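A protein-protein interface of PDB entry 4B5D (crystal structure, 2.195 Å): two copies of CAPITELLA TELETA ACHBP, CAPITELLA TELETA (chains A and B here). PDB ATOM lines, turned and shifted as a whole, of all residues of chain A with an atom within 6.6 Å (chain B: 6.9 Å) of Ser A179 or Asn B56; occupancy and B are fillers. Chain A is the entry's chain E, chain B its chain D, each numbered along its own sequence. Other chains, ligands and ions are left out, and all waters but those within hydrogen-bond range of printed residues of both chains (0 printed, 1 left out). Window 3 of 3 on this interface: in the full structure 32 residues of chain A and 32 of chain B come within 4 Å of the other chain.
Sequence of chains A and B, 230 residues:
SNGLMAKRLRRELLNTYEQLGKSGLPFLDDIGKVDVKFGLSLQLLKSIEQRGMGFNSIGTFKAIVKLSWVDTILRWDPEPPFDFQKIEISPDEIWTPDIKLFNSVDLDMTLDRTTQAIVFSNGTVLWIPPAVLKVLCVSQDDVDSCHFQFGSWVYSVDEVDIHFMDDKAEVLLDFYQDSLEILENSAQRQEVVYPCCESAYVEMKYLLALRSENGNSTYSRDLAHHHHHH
The side-chain carboxylate (OD2) of Asp A178 is in salt-bridge range of the guanidinium group (NH1) of Arg B51 (2.9 Å). The side-chain hydroxyl (OG) of Ser A179 sits at hydrogen-bond distance from the side-chain amide oxygen (OD1) of Asn B56, at 3.0 Å.
Tyr A176 touches none of the printed residues of chain B. Printed residues of chain B within 4 Å of Asp A178: Arg B51 (2.9 Å) and Leu B136 (3.5 Å). Ser A179 touches just one residue of chain B: Asn B56. Phe B55 touches none of the printed residues of chain A. Asn B56 touches just one residue of chain A: Ser A179 (3.0 Å). Printed residues of chain A within 4 Å of Leu B136: Asp A178 (3.5 Å).
No position is printed for both chains.
O of Asn B56 sits at hydrogen-bond distance from N of Arg B51. O of Cys B137 lies within hydrogen-bond range of ND2 of Asn B56, 3.0 Å away. The side-chain hydroxyl of Tyr A176 is in hydrogen-bond range of the backbone carbonyl oxygen of Leu A180 (2.9 Å).
Of the 6 printed residues of chain A, 3 touch a printed residue of chain B. Printed residues of chain A that touch a printed residue of chain B: Asp A178, Ser A179 and Leu A180. Printed residues of chain B that touch a printed residue of chain A: Arg B51, Asn B56 and Leu B136. Hydrophobic or aromatic side chains of chain B that line the printed part of chain A: Leu B136. Among the printed residues, Asp or Glu carboxylates within 4 Å of a Lys or Arg side-chain nitrogen of the other chain: Asp A178 with Arg B51 (2.9 Å).
Leu B136 touches Asp A178. NH2 of Arg B51 touches CG of Leu A180, 3.8 Å away.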
ATOM      1  N   TYR A 176      14.975   6.811   8.457  1.00  0.00           N
ATOM      2  CA  TYR A 176      16.013   6.947   9.470  1.00  0.00           C
ATOM      3  C   TYR A 176      15.461   7.103  10.881  1.00  0.00           C
ATOM      4  O   TYR A 176      14.792   8.088  11.183  1.00  0.00           O
ATOM      5  CB  TYR A 176      16.945   8.109   9.136  1.00  0.00           C
ATOM      6  CG  TYR A 176      18.149   8.203  10.049  1.00  0.00           C
ATOM      7  CD1 TYR A 176      19.103   7.200  10.076  1.00  0.00           C
ATOM      8  CD2 TYR A 176      18.334   9.299  10.879  1.00  0.00           C
ATOM      9  CE1 TYR A 176      20.215   7.284  10.908  1.00  0.00           C
ATOM     10  CE2 TYR A 176      19.437   9.393  11.712  1.00  0.00           C
ATOM     11  CZ  TYR A 176      20.372   8.384  11.722  1.00  0.00           C
ATOM     12  OH  TYR A 176      21.471   8.475  12.544  1.00  0.00           O
ATOM     13  N   GLN A 177      15.770   6.136  11.744  1.00  0.00           N
ATOM     14  CA  GLN A 177      15.276   6.140  13.118  1.00  0.00           C
ATOM     15  C   GLN A 177      16.380   6.167  14.159  1.00  0.00           C
ATOM     16  O   GLN A 177      16.156   5.764  15.294  1.00  0.00           O
ATOM     17  CB  GLN A 177      14.456   4.885  13.401  1.00  0.00           C
ATOM     18  CG  GLN A 177      13.415   4.520  12.391  1.00  0.00           C
ATOM     19  CD  GLN A 177      12.482   3.466  12.940  1.00  0.00           C
ATOM     20  OE1 GLN A 177      12.411   3.267  14.155  1.00  0.00           O
ATOM     21  NE2 GLN A 177      11.766   2.777  12.053  1.00  0.00           N
ATOM     22  N   ASP A 178      17.574   6.599  13.793  1.00  0.00           N
ATOM     23  CA  ASP A 178      18.653   6.603  14.774  1.00  0.00           C
ATOM     24  C   ASP A 178      18.856   8.012  15.334  1.00  0.00           C
ATOM     25  O   ASP A 178      18.235   8.963  14.868  1.00  0.00           O
ATOM     26  CB  ASP A 178      19.948   6.048  14.168  1.00  0.00           C
ATOM     27  CG  ASP A 178      20.743   5.206  15.153  1.00  0.00           C
ATOM     28  OD1 ASP A 178      20.653   5.479  16.362  1.00  0.00           O
ATOM     29  OD2 ASP A 178      21.454   4.267  14.725  1.00  0.00           O
ATOM     30  N   SER A 179      19.712   8.135  16.343  1.00  0.00           N
ATOM     31  CA  SER A 179      20.048   9.435  16.913  1.00  0.00           C
ATOM     32  C   SER A 179      21.423   9.915  16.439  1.00  0.00           C
ATOM     33  O   SER A 179      21.901  10.958  16.870  1.00  0.00           O
ATOM     34  CB  SER A 179      20.048   9.353  18.439  1.00  0.00           C
ATOM     35  OG  SER A 179      21.085   8.495  18.895  1.00  0.00           O
ATOM     36  N   LEU A 180      22.057   9.145  15.556  1.00  0.00           N
ATOM     37  CA  LEU A 180      23.421   9.441  15.116  1.00  0.00           C
ATOM     38  C   LEU A 180      23.535  10.666  14.222  1.00  0.00           C
ATOM     39  O   LEU A 180      22.661  10.948  13.401  1.00  0.00           O
ATOM     40  CB  LEU A 180      24.026   8.240  14.388  1.00  0.00           C
ATOM     41  CG  LEU A 180      24.426   7.048  15.251  1.00  0.00           C
ATOM     42  CD1 LEU A 180      24.922   5.951  14.356  1.00  0.00           C
ATOM     43  CD2 LEU A 180      25.492   7.460  16.258  1.00  0.00           C
ATOM     44  N   GLU A 181      24.645  11.373  14.382  1.00  0.00           N
ATOM     45  CA  GLU A 181      24.936  12.556  13.597  1.00  0.00           C
ATOM     46  C   GLU A 181      25.652  12.128  12.317  1.00  0.00           C
ATOM     47  O   GLU A 181      26.708  11.503  12.373  1.00  0.00           O
ATOM     48  CB  GLU A 181      25.812  13.503  14.413  1.00  0.00           C
ATOM     49  CG  GLU A 181      25.949  14.899  13.833  1.00  0.00           C
ATOM     50  CD  GLU A 181      26.951  15.763  14.597  1.00  0.00           C
ATOM     51  OE1 GLU A 181      27.662  15.239  15.493  1.00  0.00           O
ATOM     52  OE2 GLU A 181      27.027  16.972  14.293  1.00  0.00           O
ATOM     53  N   ILE B  48      19.562  -6.393  27.704  1.00  0.00           N
ATOM     54  CA  ILE B  48      19.677  -5.014  27.293  1.00  0.00           C
ATOM     55  C   ILE B  48      21.175  -4.674  27.203  1.00  0.00           C
ATOM     56  O   ILE B  48      21.882  -4.623  28.202  1.00  0.00           O
ATOM     57  CB  ILE B  48      18.862  -4.088  28.230  1.00  0.00           C
ATOM     58  CG1 ILE B  48      19.033  -2.630  27.834  1.00  0.00           C
ATOM     59  CG2 ILE B  48      19.204  -4.337  29.691  1.00  0.00           C
ATOM     60  CD1 ILE B  48      18.011  -2.183  26.835  1.00  0.00           C
ATOM     61  N   GLU B  49      21.661  -4.496  25.983  1.00  0.00           N
ATOM     62  CA  GLU B  49      23.084  -4.275  25.758  1.00  0.00           C
ATOM     63  C   GLU B  49      23.356  -2.884  25.221  1.00  0.00           C
ATOM     64  O   GLU B  49      22.801  -2.491  24.201  1.00  0.00           O
ATOM     65  CB  GLU B  49      23.630  -5.298  24.767  1.00  0.00           C
ATOM     66  CG  GLU B  49      23.731  -6.710  25.297  1.00  0.00           C
ATOM     67  CD  GLU B  49      24.361  -7.654  24.281  1.00  0.00           C
ATOM     68  OE1 GLU B  49      24.390  -7.296  23.081  1.00  0.00           O
ATOM     69  OE2 GLU B  49      24.826  -8.746  24.681  1.00  0.00           O
ATOM     70  N   GLN B  50      24.235  -2.155  25.893  1.00  0.00           N
ATOM     71  CA  GLN B  50      24.562  -0.785  25.506  1.00  0.00           C
ATOM     72  C   GLN B  50      25.255  -0.758  24.155  1.00  0.00           C
ATOM     73  O   GLN B  50      26.108  -1.604  23.878  1.00  0.00           O
ATOM     74  CB  GLN B  50      25.465  -0.148  26.567  1.00  0.00           C
ATOM     75  CG  GLN B  50      26.124   1.155  26.164  1.00  0.00           C
ATOM     76  CD  GLN B  50      27.107   1.647  27.220  1.00  0.00           C
ATOM     77  OE1 GLN B  50      27.798   0.851  27.866  1.00  0.00           O
ATOM     78  NE2 GLN B  50      27.167   2.961  27.408  1.00  0.00           N
ATOM     79  N   ARG B  51      24.877   0.197  23.306  1.00  0.00           N
ATOM     80  CA  ARG B  51      25.568   0.371  22.026  1.00  0.00           C
ATOM     81  C   ARG B  51      26.720   1.356  22.188  1.00  0.00           C
ATOM     82  O   ARG B  51      26.509   2.528  22.512  1.00  0.00           O
ATOM     83  CB  ARG B  51      24.610   0.834  20.925  1.00  0.00           C
ATOM     84  CG  ARG B  51      25.265   0.976  19.568  1.00  0.00           C
ATOM     85  CD  ARG B  51      24.291   1.500  18.529  1.00  0.00           C
ATOM     86  NE  ARG B  51      24.091   2.940  18.656  1.00  0.00           N
ATOM     87  CZ  ARG B  51      23.170   3.635  17.991  1.00  0.00           C
ATOM     88  NH1 ARG B  51      22.358   3.029  17.138  1.00  0.00           N
ATOM     89  NH2 ARG B  51      23.070   4.946  18.175  1.00  0.00           N
ATOM     90  N   GLY B  52      27.938   0.871  21.963  1.00  0.00           N
ATOM     91  CA  GLY B  52      29.130   1.659  22.215  1.00  0.00           C
ATOM     92  C   GLY B  52      29.189   2.169  23.647  1.00  0.00           C
ATOM     93  O   GLY B  52      28.943   1.427  24.602  1.00  0.00           O
ATOM     94  N   MET B  53      29.516   3.449  23.790  1.00  0.00           N
ATOM     95  CA  MET B  53      29.556   4.094  25.095  1.00  0.00           C
ATOM     96  C   MET B  53      28.489   5.183  25.170  1.00  0.00           C
ATOM     97  O   MET B  53      28.544   6.069  26.025  1.00  0.00           O
ATOM     98  CB  MET B  53      30.943   4.693  25.357  1.00  0.00           C
ATOM     99  CG  MET B  53      32.075   3.678  25.358  1.00  0.00           C
ATOM    100  SD  MET B  53      33.671   4.441  25.700  1.00  0.00           S
ATOM    101  CE  MET B  53      33.858   5.545  24.299  1.00  0.00           C
ATOM    102  N   GLY B  54      27.516   5.103  24.266  1.00  0.00           N
ATOM    103  CA  GLY B  54      26.457   6.090  24.187  1.00  0.00           C
ATOM    104  C   GLY B  54      25.231   5.734  25.012  1.00  0.00           C
ATOM    105  O   GLY B  54      25.257   4.821  25.840  1.00  0.00           O
ATOM    106  N   PHE B  55      24.142   6.453  24.770  1.00  0.00           N
ATOM    107  CA  PHE B  55      22.951   6.311  25.595  1.00  0.00           C
ATOM    108  C   PHE B  55      21.894   5.438  24.919  1.00  0.00           C
ATOM    109  O   PHE B  55      20.767   5.315  25.398  1.00  0.00           O
ATOM    110  CB  PHE B  55      22.414   7.694  25.974  1.00  0.00           C
ATOM    111  CG  PHE B  55      23.501   8.692  26.288  1.00  0.00           C
ATOM    112  CD1 PHE B  55      24.303   8.540  27.414  1.00  0.00           C
ATOM    113  CD2 PHE B  55      23.736   9.773  25.446  1.00  0.00           C
ATOM    114  CE1 PHE B  55      25.315   9.454  27.699  1.00  0.00           C
ATOM    115  CE2 PHE B  55      24.744  10.694  25.730  1.00  0.00           C
ATOM    116  CZ  PHE B  55      25.533  10.531  26.855  1.00  0.00           C
ATOM    117  N   ASN B  56      22.274   4.814  23.809  1.00  0.00           N
ATOM    118  CA  ASN B  56      21.420   3.817  23.181  1.00  0.00           C
ATOM    119  C   ASN B  56      21.824   2.392  23.520  1.00  0.00           C
ATOM    120  O   ASN B  56      22.937   2.127  23.991  1.00  0.00           O
ATOM    121  CB  ASN B  56      21.343   4.017  21.673  1.00  0.00           C
ATOM    122  CG  ASN B  56      20.626   5.294  21.307  1.00  0.00           C
ATOM    123  OD1 ASN B  56      21.250   6.271  20.892  1.00  0.00           O
ATOM    124  ND2 ASN B  56      19.306   5.300  21.474  1.00  0.00           N
ATOM    125  N   SER B  57      20.895   1.480  23.287  1.00  0.00           N
ATOM    126  CA  SER B  57      21.093   0.099  23.653  1.00  0.00           C
ATOM    127  C   SER B  57      20.223  -0.795  22.795  1.00  0.00           C
ATOM    128  O   SER B  57      19.242  -0.348  22.194  1.00  0.00           O
ATOM    129  CB  SER B  57      20.723  -0.096  25.121  1.00  0.00           C
ATOM    130  OG  SER B  57      19.427   0.421  25.355  1.00  0.00           O
ATOM    131  N   ILE B  58      20.583  -2.068  22.755  1.00  0.00           N
ATOM    132  CA  ILE B  58      19.791  -3.049  22.047  1.00  0.00           C
ATOM    133  C   ILE B  58      19.017  -3.930  23.027  1.00  0.00           C
ATOM    134  O   ILE B  58      19.600  -4.662  23.833  1.00  0.00           O
ATOM    135  CB  ILE B  58      20.673  -3.888  21.119  1.00  0.00           C
ATOM    136  CG1 ILE B  58      21.263  -2.995  20.026  1.00  0.00           C
ATOM    137  CG2 ILE B  58      19.873  -5.021  20.507  1.00  0.00           C
ATOM    138  CD1 ILE B  58      22.464  -3.596  19.345  1.00  0.00           C
ATOM    139  N   LEU B 136      16.047  -0.977  19.103  1.00  0.00           N
ATOM    140  CA  LEU B 136      16.929   0.033  19.653  1.00  0.00           C
ATOM    141  C   LEU B 136      16.209   0.777  20.792  1.00  0.00           C
ATOM    142  O   LEU B 136      15.076   1.250  20.618  1.00  0.00           O
ATOM    143  CB  LEU B 136      17.332   1.005  18.544  1.00  0.00           C
ATOM    144  CG  LEU B 136      18.613   1.803  18.750  1.00  0.00           C
ATOM    145  CD1 LEU B 136      19.787   0.851  18.865  1.00  0.00           C
ATOM    146  CD2 LEU B 136      18.802   2.746  17.581  1.00  0.00           C
ATOM    147  N   CYS B 137      16.859   0.858  21.955  1.00  0.00           N
ATOM    148  CA  CYS B 137      16.303   1.571  23.105  1.00  0.00           C
ATOM    149  C   CYS B 137      17.143   2.780  23.488  1.00  0.00           C
ATOM    150  O   CYS B 137      18.248   2.986  22.980  1.00  0.00           O
ATOM    151  CB  CYS B 137      16.216   0.651  24.329  1.00  0.00           C
ATOM    152  SG  CYS B 137      15.323  -0.891  24.081  1.00  0.00           S
ATOM    153  N   VAL B 138      16.601   3.575  24.400  1.00  0.00           N
ATOM    154  CA  VAL B 138      17.347   4.632  25.058  1.00  0.00           C
ATOM    155  C   VAL B 138      17.554   4.205  26.503  1.00  0.00           C
ATOM    156  O   VAL B 138      16.607   3.818  27.187  1.00  0.00           O
ATOM    157  CB  VAL B 138      16.590   5.974  25.047  1.00  0.00           C
ATOM    158  CG1 VAL B 138      17.400   7.044  25.786  1.00  0.00           C
ATOM    159  CG2 VAL B 138      16.274   6.407  23.614  1.00  0.00           C
ATOM    160  N   SER B 139      18.798   4.246  26.959  1.00  0.00           N
ATOM    161  CA  SER B 139      19.107   3.877  28.330  1.00  0.00           C
ATOM    162  C   SER B 139      19.765   5.060  29.017  1.00  0.00           C
ATOM    163  O   SER B 139      20.949   5.331  28.820  1.00  0.00           O
ATOM    164  CB  SER B 139      20.003   2.640  28.367  1.00  0.00           C
ATOM    165  OG  SER B 139      19.291   1.507  27.902  1.00  0.00           O
